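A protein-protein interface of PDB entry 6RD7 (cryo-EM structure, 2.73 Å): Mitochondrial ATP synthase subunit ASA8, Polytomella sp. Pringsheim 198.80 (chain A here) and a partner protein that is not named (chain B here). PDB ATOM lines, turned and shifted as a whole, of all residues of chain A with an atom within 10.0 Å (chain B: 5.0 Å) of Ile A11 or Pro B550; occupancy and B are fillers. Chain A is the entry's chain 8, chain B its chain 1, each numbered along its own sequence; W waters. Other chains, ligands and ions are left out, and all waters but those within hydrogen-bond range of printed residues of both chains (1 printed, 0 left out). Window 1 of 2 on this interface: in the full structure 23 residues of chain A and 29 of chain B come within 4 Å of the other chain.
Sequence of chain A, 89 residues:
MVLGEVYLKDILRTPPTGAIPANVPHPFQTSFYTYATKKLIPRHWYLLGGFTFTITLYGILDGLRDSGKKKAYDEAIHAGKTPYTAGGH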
ATOM      1  N   LEU A   3      25.704 -23.725 -29.423  1.00  0.00           N
ATOM      2  CA  LEU A   3      25.015 -22.864 -28.477  1.00  0.00           C
ATOM      3  C   LEU A   3      23.947 -23.672 -27.755  1.00  0.00           C
ATOM      4  O   LEU A   3      23.003 -24.159 -28.381  1.00  0.00           O
ATOM      5  CB  LEU A   3      24.407 -21.661 -29.198  1.00  0.00           C
ATOM      6  CG  LEU A   3      23.966 -20.450 -28.380  1.00  0.00           C
ATOM      7  CD1 LEU A   3      24.300 -19.196 -29.150  1.00  0.00           C
ATOM      8  CD2 LEU A   3      22.480 -20.494 -28.065  1.00  0.00           C
ATOM      9  N   GLY A   4      24.092 -23.830 -26.444  1.00  0.00           N
ATOM     10  CA  GLY A   4      23.141 -24.572 -25.648  1.00  0.00           C
ATOM     11  C   GLY A   4      22.135 -23.665 -24.975  1.00  0.00           C
ATOM     12  O   GLY A   4      22.036 -22.471 -25.260  1.00  0.00           O
ATOM     13  N   GLU A   5      21.354 -24.265 -24.072  1.00  0.00           N
ATOM     14  CA  GLU A   5      20.362 -23.510 -23.311  1.00  0.00           C
ATOM     15  C   GLU A   5      21.024 -22.511 -22.374  1.00  0.00           C
ATOM     16  O   GLU A   5      20.464 -21.444 -22.095  1.00  0.00           O
ATOM     17  CB  GLU A   5      19.483 -24.465 -22.507  1.00  0.00           C
ATOM     18  CG  GLU A   5      18.354 -25.105 -23.277  1.00  0.00           C
ATOM     19  CD  GLU A   5      17.180 -25.460 -22.383  1.00  0.00           C
ATOM     20  OE1 GLU A   5      16.694 -26.607 -22.462  1.00  0.00           O
ATOM     21  OE2 GLU A   5      16.743 -24.590 -21.601  1.00  0.00           O
ATOM     22  N   VAL A   6      22.238 -22.828 -21.914  1.00  0.00           N
ATOM     23  CA  VAL A   6      22.901 -22.048 -20.873  1.00  0.00           C
ATOM     24  C   VAL A   6      23.315 -20.677 -21.401  1.00  0.00           C
ATOM     25  O   VAL A   6      23.472 -19.718 -20.636  1.00  0.00           O
ATOM     26  CB  VAL A   6      24.094 -22.854 -20.312  1.00  0.00           C
ATOM     27  CG1 VAL A   6      25.193 -23.026 -21.354  1.00  0.00           C
ATOM     28  CG2 VAL A   6      24.634 -22.254 -19.019  1.00  0.00           C
ATOM     29  N   TYR A   7      23.446 -20.544 -22.720  1.00  0.00           N
ATOM     30  CA  TYR A   7      23.805 -19.250 -23.282  1.00  0.00           C
ATOM     31  C   TYR A   7      22.594 -18.335 -23.379  1.00  0.00           C
ATOM     32  O   TYR A   7      22.741 -17.119 -23.532  1.00  0.00           O
ATOM     33  CB  TYR A   7      24.464 -19.438 -24.645  1.00  0.00           C
ATOM     34  CG  TYR A   7      25.893 -19.899 -24.536  1.00  0.00           C
ATOM     35  CD1 TYR A   7      26.857 -19.090 -23.955  1.00  0.00           C
ATOM     36  CD2 TYR A   7      26.274 -21.151 -24.993  1.00  0.00           C
ATOM     37  CE1 TYR A   7      28.163 -19.509 -23.843  1.00  0.00           C
ATOM     38  CE2 TYR A   7      27.579 -21.578 -24.886  1.00  0.00           C
ATOM     39  CZ  TYR A   7      28.517 -20.753 -24.310  1.00  0.00           C
ATOM     40  OH  TYR A   7      29.817 -21.178 -24.203  1.00  0.00           O
ATOM     41  N   LEU A   8      21.389 -18.891 -23.278  1.00  0.00           N
ATOM     42  CA  LEU A   8      20.205 -18.043 -23.288  1.00  0.00           C
ATOM     43  C   LEU A   8      19.317 -18.342 -22.090  1.00  0.00           C
ATOM     44  O   LEU A   8      18.090 -18.290 -22.190  1.00  0.00           O
ATOM     45  CB  LEU A   8      19.460 -18.187 -24.622  1.00  0.00           C
ATOM     46  CG  LEU A   8      19.051 -19.511 -25.277  1.00  0.00           C
ATOM     47  CD1 LEU A   8      17.702 -20.040 -24.847  1.00  0.00           C
ATOM     48  CD2 LEU A   8      19.040 -19.325 -26.769  1.00  0.00           C
ATOM     49  N   LYS A   9      19.948 -18.574 -20.936  1.00  0.00           N
ATOM     50  CA  LYS A   9      19.248 -19.113 -19.773  1.00  0.00           C
ATOM     51  C   LYS A   9      18.235 -18.124 -19.212  1.00  0.00           C
ATOM     52  O   LYS A   9      17.055 -18.453 -19.046  1.00  0.00           O
ATOM     53  CB  LYS A   9      20.259 -19.504 -18.699  1.00  0.00           C
ATOM     54  CG  LYS A   9      19.627 -19.882 -17.379  1.00  0.00           C
ATOM     55  CD  LYS A   9      20.675 -20.118 -16.308  1.00  0.00           C
ATOM     56  CE  LYS A   9      21.354 -18.822 -15.902  1.00  0.00           C
ATOM     57  NZ  LYS A   9      20.690 -18.181 -14.734  1.00  0.00           N
ATOM     58  N   ASP A  10      18.671 -16.906 -18.918  1.00  0.00           N
ATOM     59  CA  ASP A  10      17.754 -15.871 -18.479  1.00  0.00           C
ATOM     60  C   ASP A  10      17.595 -14.743 -19.476  1.00  0.00           C
ATOM     61  O   ASP A  10      16.952 -13.747 -19.146  1.00  0.00           O
ATOM     62  CB  ASP A  10      18.202 -15.283 -17.135  1.00  0.00           C
ATOM     63  CG  ASP A  10      17.972 -16.233 -15.984  1.00  0.00           C
ATOM     64  OD1 ASP A  10      16.918 -16.897 -15.963  1.00  0.00           O
ATOM     65  OD2 ASP A  10      18.846 -16.320 -15.097  1.00  0.00           O
ATOM     66  N   ILE A  11      18.141 -14.875 -20.681  1.00  0.00           N
ATOM     67  CA  ILE A  11      18.125 -13.775 -21.636  1.00  0.00           C
ATOM     68  C   ILE A  11      16.930 -13.896 -22.571  1.00  0.00           C
ATOM     69  O   ILE A  11      16.162 -12.946 -22.750  1.00  0.00           O
ATOM     70  CB  ILE A  11      19.447 -13.739 -22.417  1.00  0.00           C
ATOM     71  CG1 ILE A  11      20.626 -13.620 -21.458  1.00  0.00           C
ATOM     72  CG2 ILE A  11      19.440 -12.599 -23.380  1.00  0.00           C
ATOM     73  CD1 ILE A  11      21.923 -14.087 -22.046  1.00  0.00           C
ATOM     74  N   LEU A  12      16.759 -15.062 -23.181  1.00  0.00           N
ATOM     75  CA  LEU A  12      15.697 -15.303 -24.145  1.00  0.00           C
ATOM     76  C   LEU A  12      14.964 -16.579 -23.781  1.00  0.00           C
ATOM     77  O   LEU A  12      15.587 -17.622 -23.571  1.00  0.00           O
ATOM     78  CB  LEU A  12      16.243 -15.430 -25.562  1.00  0.00           C
ATOM     79  CG  LEU A  12      16.797 -14.169 -26.212  1.00  0.00           C
ATOM     80  CD1 LEU A  12      17.562 -14.546 -27.453  1.00  0.00           C
ATOM     81  CD2 LEU A  12      15.673 -13.213 -26.541  1.00  0.00           C
ATOM     82  N   ARG A  13      13.642 -16.497 -23.700  1.00  0.00           N
ATOM     83  CA  ARG A  13      12.811 -17.663 -23.464  1.00  0.00           C
ATOM     84  C   ARG A  13      11.755 -17.751 -24.554  1.00  0.00           C
ATOM     85  O   ARG A  13      11.339 -16.746 -25.130  1.00  0.00           O
ATOM     86  CB  ARG A  13      12.147 -17.622 -22.083  1.00  0.00           C
ATOM     87  CG  ARG A  13      13.097 -17.307 -20.952  1.00  0.00           C
ATOM     88  CD  ARG A  13      12.552 -17.746 -19.626  1.00  0.00           C
ATOM     89  NE  ARG A  13      13.364 -17.240 -18.529  1.00  0.00           N
ATOM     90  CZ  ARG A  13      13.104 -16.122 -17.869  1.00  0.00           C
ATOM     91  NH1 ARG A  13      13.896 -15.732 -16.885  1.00  0.00           N
ATOM     92  NH2 ARG A  13      12.050 -15.393 -18.194  1.00  0.00           N
ATOM     93  N   THR A  14      11.342 -18.962 -24.833  1.00  0.00           N
ATOM     94  CA  THR A  14      10.280 -19.298 -25.764  1.00  0.00           C
ATOM     95  C   THR A  14       8.931 -19.083 -25.089  1.00  0.00           C
ATOM     96  O   THR A  14       8.883 -18.825 -23.883  1.00  0.00           O
ATOM     97  CB  THR A  14      10.446 -20.749 -26.212  1.00  0.00           C
ATOM     98  OG1 THR A  14      10.525 -21.589 -25.062  1.00  0.00           O
ATOM     99  CG2 THR A  14      11.696 -20.896 -27.050  1.00  0.00           C
ATOM    100  N   ALA A  22       3.439 -16.199 -13.445  1.00  0.00           N
ATOM    101  CA  ALA A  22       2.921 -15.000 -12.810  1.00  0.00           C
ATOM    102  C   ALA A  22       3.529 -13.777 -13.477  1.00  0.00           C
ATOM    103  O   ALA A  22       4.623 -13.841 -14.041  1.00  0.00           O
ATOM    104  CB  ALA A  22       3.237 -15.003 -11.318  1.00  0.00           C
ATOM    105  N   ASN A  23       2.806 -12.663 -13.431  1.00  0.00           N
ATOM    106  CA  ASN A  23       3.311 -11.437 -14.026  1.00  0.00           C
ATOM    107  C   ASN A  23       4.444 -10.872 -13.185  1.00  0.00           C
ATOM    108  O   ASN A  23       4.389 -10.886 -11.954  1.00  0.00           O
ATOM    109  CB  ASN A  23       2.189 -10.414 -14.169  1.00  0.00           C
ATOM    110  CG  ASN A  23       2.524  -9.326 -15.159  1.00  0.00           C
ATOM    111  OD1 ASN A  23       3.573  -9.357 -15.796  1.00  0.00           O
ATOM    112  ND2 ASN A  23       1.635  -8.358 -15.298  1.00  0.00           N
ATOM    113  N   VAL A  24       5.483 -10.394 -13.859  1.00  0.00           N
ATOM    114  CA  VAL A  24       6.629  -9.784 -13.194  1.00  0.00           C
ATOM    115  C   VAL A  24       6.200  -8.411 -12.696  1.00  0.00           C
ATOM    116  O   VAL A  24       5.737  -7.584 -13.491  1.00  0.00           O
ATOM    117  CB  VAL A  24       7.838  -9.692 -14.137  1.00  0.00           C
ATOM    118  CG1 VAL A  24       8.889  -8.762 -13.570  1.00  0.00           C
ATOM    119  CG2 VAL A  24       8.421 -11.068 -14.371  1.00  0.00           C
ATOM    120  N   PRO A  25       6.320  -8.130 -11.405  1.00  0.00           N
ATOM    121  CA  PRO A  25       5.904  -6.823 -10.899  1.00  0.00           C
ATOM    122  C   PRO A  25       6.920  -5.737 -11.201  1.00  0.00           C
ATOM    123  O   PRO A  25       8.128  -5.971 -11.262  1.00  0.00           O
ATOM    124  CB  PRO A  25       5.791  -7.055  -9.390  1.00  0.00           C
ATOM    125  CG  PRO A  25       6.737  -8.141  -9.116  1.00  0.00           C
ATOM    126  CD  PRO A  25       6.761  -9.022 -10.323  1.00  0.00           C
ATOM    127  N   VAL B 545       4.775 -12.045 -21.917  1.00  0.00           N
ATOM    128  CA  VAL B 545       5.743 -11.084 -22.437  1.00  0.00           C
ATOM    129  C   VAL B 545       6.943 -10.968 -21.505  1.00  0.00           C
ATOM    130  O   VAL B 545       8.096 -11.012 -21.947  1.00  0.00           O
ATOM    131  CB  VAL B 545       5.053  -9.723 -22.650  1.00  0.00           C
ATOM    132  CG1 VAL B 545       6.058  -8.612 -22.757  1.00  0.00           C
ATOM    133  CG2 VAL B 545       4.199  -9.759 -23.880  1.00  0.00           C
ATOM    134  N   ALA B 546       6.691 -10.851 -20.200  1.00  0.00           N
ATOM    135  CA  ALA B 546       7.781 -10.718 -19.239  1.00  0.00           C
ATOM    136  C   ALA B 546       8.538 -12.026 -19.066  1.00  0.00           C
ATOM    137  O   ALA B 546       9.696 -12.026 -18.637  1.00  0.00           O
ATOM    138  CB  ALA B 546       7.237 -10.233 -17.899  1.00  0.00           C
ATOM    139  N   HIS B 547       7.899 -13.150 -19.383  1.00  0.00           N
ATOM    140  CA  HIS B 547       8.586 -14.431 -19.334  1.00  0.00           C
ATOM    141  C   HIS B 547       9.485 -14.618 -20.543  1.00  0.00           C
ATOM    142  O   HIS B 547      10.619 -15.089 -20.412  1.00  0.00           O
ATOM    143  CB  HIS B 547       7.563 -15.559 -19.247  1.00  0.00           C
ATOM    144  CG  HIS B 547       8.147 -16.921 -19.441  1.00  0.00           C
ATOM    145  ND1 HIS B 547       8.813 -17.593 -18.441  1.00  0.00           N
ATOM    146  CD2 HIS B 547       8.166 -17.735 -20.521  1.00  0.00           C
ATOM    147  CE1 HIS B 547       9.218 -18.763 -18.897  1.00  0.00           C
ATOM    148  NE2 HIS B 547       8.841 -18.873 -20.157  1.00  0.00           N
ATOM    149  N   MET B 548       8.996 -14.253 -21.729  1.00  0.00           N
ATOM    150  CA  MET B 548       9.766 -14.475 -22.948  1.00  0.00           C
ATOM    151  C   MET B 548      10.941 -13.518 -23.057  1.00  0.00           C
ATOM    152  O   MET B 548      12.045 -13.925 -23.430  1.00  0.00           O
ATOM    153  CB  MET B 548       8.862 -14.334 -24.163  1.00  0.00           C
ATOM    154  CG  MET B 548       8.141 -15.590 -24.533  1.00  0.00           C
ATOM    155  SD  MET B 548       7.453 -15.408 -26.166  1.00  0.00           S
ATOM    156  CE  MET B 548       6.028 -14.434 -25.759  1.00  0.00           C
ATOM    157  N   ASP B 549      10.730 -12.244 -22.751  1.00  0.00           N
ATOM    158  CA  ASP B 549      11.786 -11.239 -22.815  1.00  0.00           C
ATOM    159  C   ASP B 549      11.869 -10.532 -21.472  1.00  0.00           C
ATOM    160  O   ASP B 549      11.319  -9.439 -21.301  1.00  0.00           O
ATOM    161  CB  ASP B 549      11.539 -10.247 -23.950  1.00  0.00           C
ATOM    162  CG  ASP B 549      12.828  -9.764 -24.585  1.00  0.00           C
ATOM    163  OD1 ASP B 549      13.902  -9.980 -23.987  1.00  0.00           O
ATOM    164  OD2 ASP B 549      12.770  -9.180 -25.685  1.00  0.00           O
ATOM    165  N   PRO B 550      12.554 -11.128 -20.493  1.00  0.00           N
ATOM    166  CA  PRO B 550      12.667 -10.474 -19.185  1.00  0.00           C
ATOM    167  C   PRO B 550      13.591  -9.275 -19.179  1.00  0.00           C
ATOM    168  O   PRO B 550      13.392  -8.369 -18.362  1.00  0.00           O
ATOM    169  CB  PRO B 550      13.207 -11.588 -18.283  1.00  0.00           C
ATOM    170  CG  PRO B 550      13.923 -12.482 -19.191  1.00  0.00           C
ATOM    171  CD  PRO B 550      13.250 -12.425 -20.520  1.00  0.00           C
ATOM    172  N   LEU B 551      14.576  -9.223 -20.073  1.00  0.00           N
ATOM    173  CA  LEU B 551      15.511  -8.109 -20.068  1.00  0.00           C
ATOM    174  C   LEU B 551      14.912  -6.867 -20.704  1.00  0.00           C
ATOM    175  O   LEU B 551      15.212  -5.752 -20.268  1.00  0.00           O
ATOM    176  CB  LEU B 551      16.807  -8.481 -20.784  1.00  0.00           C
ATOM    177  CG  LEU B 551      17.912  -9.192 -20.001  1.00  0.00           C
ATOM    178  CD1 LEU B 551      18.221  -8.410 -18.769  1.00  0.00           C
ATOM    179  CD2 LEU B 551      17.576 -10.594 -19.636  1.00  0.00           C
ATOM    180  N   LEU B 552      14.060  -7.036 -21.713  1.00  0.00           N
ATOM    181  CA  LEU B 552      13.359  -5.897 -22.292  1.00  0.00           C
ATOM    182  C   LEU B 552      12.384  -5.294 -21.296  1.00  0.00           C
ATOM    183  O   LEU B 552      12.278  -4.068 -21.184  1.00  0.00           O
ATOM    184  CB  LEU B 552      12.633  -6.326 -23.563  1.00  0.00           C
ATOM    185  CG  LEU B 552      11.717  -5.299 -24.218  1.00  0.00           C
ATOM    186  CD1 LEU B 552      12.523  -4.137 -24.756  1.00  0.00           C
ATOM    187  CD2 LEU B 552      10.903  -5.940 -25.313  1.00  0.00           C
ATOM    188  N   ILE B 553      11.694  -6.146 -20.540  1.00  0.00           N
ATOM    189  CA  ILE B 553      10.793  -5.679 -19.495  1.00  0.00           C
ATOM    190  C   ILE B 553      11.581  -5.021 -18.368  1.00  0.00           C
ATOM    191  O   ILE B 553      11.144  -4.019 -17.798  1.00  0.00           O
ATOM    192  CB  ILE B 553       9.924  -6.853 -19.008  1.00  0.00           C
ATOM    193  CG1 ILE B 553       9.030  -7.336 -20.147  1.00  0.00           C
ATOM    194  CG2 ILE B 553       9.063  -6.478 -17.828  1.00  0.00           C
ATOM    195  CD1 ILE B 553       8.217  -6.251 -20.799  1.00  0.00           C
ATOM    196  N   LYS B 554      12.781  -5.530 -18.083  1.00  0.00           N
ATOM    197  CA  LYS B 554      13.655  -4.906 -17.093  1.00  0.00           C
ATOM    198  C   LYS B 554      14.105  -3.515 -17.529  1.00  0.00           C
ATOM    199  O   LYS B 554      14.140  -2.585 -16.718  1.00  0.00           O
ATOM    200  CB  LYS B 554      14.860  -5.810 -16.845  1.00  0.00           C
ATOM    201  CG  LYS B 554      15.865  -5.290 -15.855  1.00  0.00           C
ATOM    202  CD  LYS B 554      17.224  -5.885 -16.126  1.00  0.00           C
ATOM    203  CE  LYS B 554      18.166  -5.664 -14.969  1.00  0.00           C
ATOM    204  NZ  LYS B 554      19.471  -6.311 -15.224  1.00  0.00           N
ATOM    205  N   HIS B 590      20.179  -7.090 -25.968  1.00  0.00           N
ATOM    206  CA  HIS B 590      20.425  -8.366 -25.317  1.00  0.00           C
ATOM    207  C   HIS B 590      20.056  -9.558 -26.185  1.00  0.00           C
ATOM    208  O   HIS B 590      20.402 -10.683 -25.822  1.00  0.00           O
ATOM    209  CB  HIS B 590      19.646  -8.435 -24.011  1.00  0.00           C
ATOM    210  CG  HIS B 590      18.170  -8.283 -24.190  1.00  0.00           C
ATOM    211  ND1 HIS B 590      17.564  -7.059 -24.355  1.00  0.00           N
ATOM    212  CD2 HIS B 590      17.180  -9.204 -24.249  1.00  0.00           C
ATOM    213  CE1 HIS B 590      16.264  -7.231 -24.502  1.00  0.00           C
ATOM    214  NE2 HIS B 590      16.005  -8.523 -24.442  1.00  0.00           N
ATOM    215  N   LEU B 593      23.192 -11.013 -27.316  1.00  0.00           N
ATOM    216  CA  LEU B 593      24.106 -11.390 -26.238  1.00  0.00           C
ATOM    217  C   LEU B 593      24.368 -12.893 -26.098  1.00  0.00           C
ATOM    218  O   LEU B 593      25.508 -13.248 -25.749  1.00  0.00           O
ATOM    219  CB  LEU B 593      23.600 -10.780 -24.926  1.00  0.00           C
ATOM    220  CG  LEU B 593      24.244 -11.182 -23.603  1.00  0.00           C
ATOM    221  CD1 LEU B 593      25.663 -10.680 -23.533  1.00  0.00           C
ATOM    222  CD2 LEU B 593      23.440 -10.646 -22.466  1.00  0.00           C
ATOM    223  N   PRO B 594      23.404 -13.821 -26.314  1.00  0.00           N
ATOM    224  CA  PRO B 594      23.794 -15.246 -26.370  1.00  0.00           C
ATOM    225  C   PRO B 594      24.822 -15.577 -27.438  1.00  0.00           C
ATOM    226  O   PRO B 594      25.769 -16.329 -27.172  1.00  0.00           O
ATOM    227  CB  PRO B 594      22.460 -15.946 -26.634  1.00  0.00           C
ATOM    228  CG  PRO B 594      21.498 -15.122 -25.960  1.00  0.00           C
ATOM    229  CD  PRO B 594      21.931 -13.723 -26.207  1.00  0.00           C
ATOM    230  N   ARG B 597      28.267 -14.053 -26.284  1.00  0.00           N
ATOM    231  CA  ARG B 597      28.901 -14.843 -25.234  1.00  0.00           C
ATOM    232  C   ARG B 597      29.403 -16.180 -25.764  1.00  0.00           C
ATOM    233  O   ARG B 597      30.492 -16.633 -25.386  1.00  0.00           O
ATOM    234  CB  ARG B 597      27.923 -15.062 -24.086  1.00  0.00           C
ATOM    235  CG  ARG B 597      27.663 -13.825 -23.278  1.00  0.00           C
ATOM    236  CD  ARG B 597      26.868 -14.150 -22.045  1.00  0.00           C
ATOM    237  NE  ARG B 597      27.704 -14.108 -20.858  1.00  0.00           N
ATOM    238  CZ  ARG B 597      27.831 -15.118 -20.013  1.00  0.00           C
ATOM    239  NH1 ARG B 597      28.613 -15.002 -18.956  1.00  0.00           N
ATOM    240  NH2 ARG B 597      27.173 -16.247 -20.225  1.00  0.00           N
HETATM  241  O   HOH W   1       9.946 -21.191 -21.646  1.00  0.00           O
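Among the printed residues, merely in contact across the chains: Leu A3 with Pro B594 (3.8 Å), Tyr A7 with Pro B594 (3.3 Å), Leu A8 with Pro B594 (3.9 Å), Asp A10 with Pro B550 (3.3 Å), Asp A10 with Leu B551 (3.3 Å), Ile A11 with Asp B549 (3.9 Å), Ile A11 with Pro B550 (3.7 Å), Ile A11 with Leu B551 (3.8 Å), Ile A11 with His B590 (3.2 Å), Ile A11 with Leu B593 (3.8 Å), Ile A11 with Pro B594 (3.9 Å), Leu A12 with Met B548 (3.96 Å), Arg A13 with Pro B550 (3.6 Å), Thr A14 with His B547 (3.6 Å), Thr A14 with Met B548 (3.4 Å) and Val A24 with Ala B546 (3.8 Å).
Of the 16 printed residues of chain A, 9 touch a printed residue of chain B. Hydrophobic or aromatic side chains of chain A that line the printed part of chain B: Leu A3, Leu A8, Ile A11 and Val A24. Printed residues of chain B that touch a printed residue of chain A: Ala B546, His B547, Met B548, Asp B549, Pro B550, Leu B551, His B590, Leu B593 and Pro B594. Among the printed residues, 18 pairs touch across the chains.
Water W1 bridges a ring nitrogen (NE2) of His B547 and the backbone carbonyl oxygen (O) of Thr A14.
Of the printed residues of chain B, Leu A8 touches Pro B594. Of chain B, only Asp B549, Pro B550, Leu B551, His B590, Leu B593 and Pro B594 come within 4 Å of Ile A11. Printed residues of chain B within 4 Å of Leu A12: Met B548 (3.96 Å). Pro A25 touches none of the printed residues of chain B. Of chain A, only Ile A11 comes within 4 Å of Asp B549. Pro B550 touches just these residues of chain A: Asp A10, Ile A11 and Arg A13. Leu B551 touches two residues of chain A. Printed residues of chain A within 4 Å of Leu B593: Ile A11. The nearest residue of chain B that does not touch Ile A11 is Met B548 (4.3 Å).
The backbone carbonyl oxygen (O) of Met B548 sits at hydrogen-bond distance from the backbone NH (N) of Arg A13, at 3.0 Å. The guanidinium group (NH2) of Arg A13 lies within hydrogen-bond range of the backbone carbonyl oxygen (O) of His B547.
The guanidinium group (NH1) of Arg A13 is in salt-bridge range of the side-chain carboxylate (OD1) of Asp A10, at 3.4 Å. The side-chain carboxylate (OD1) of Asp B549 sits at hydrogen-bond distance from a ring nitrogen (NE2) of His B590 (2.6 Å). The side-chain carboxylate of Asp A10 is in salt-bridge range of the side-chain amino group of Lys A9.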
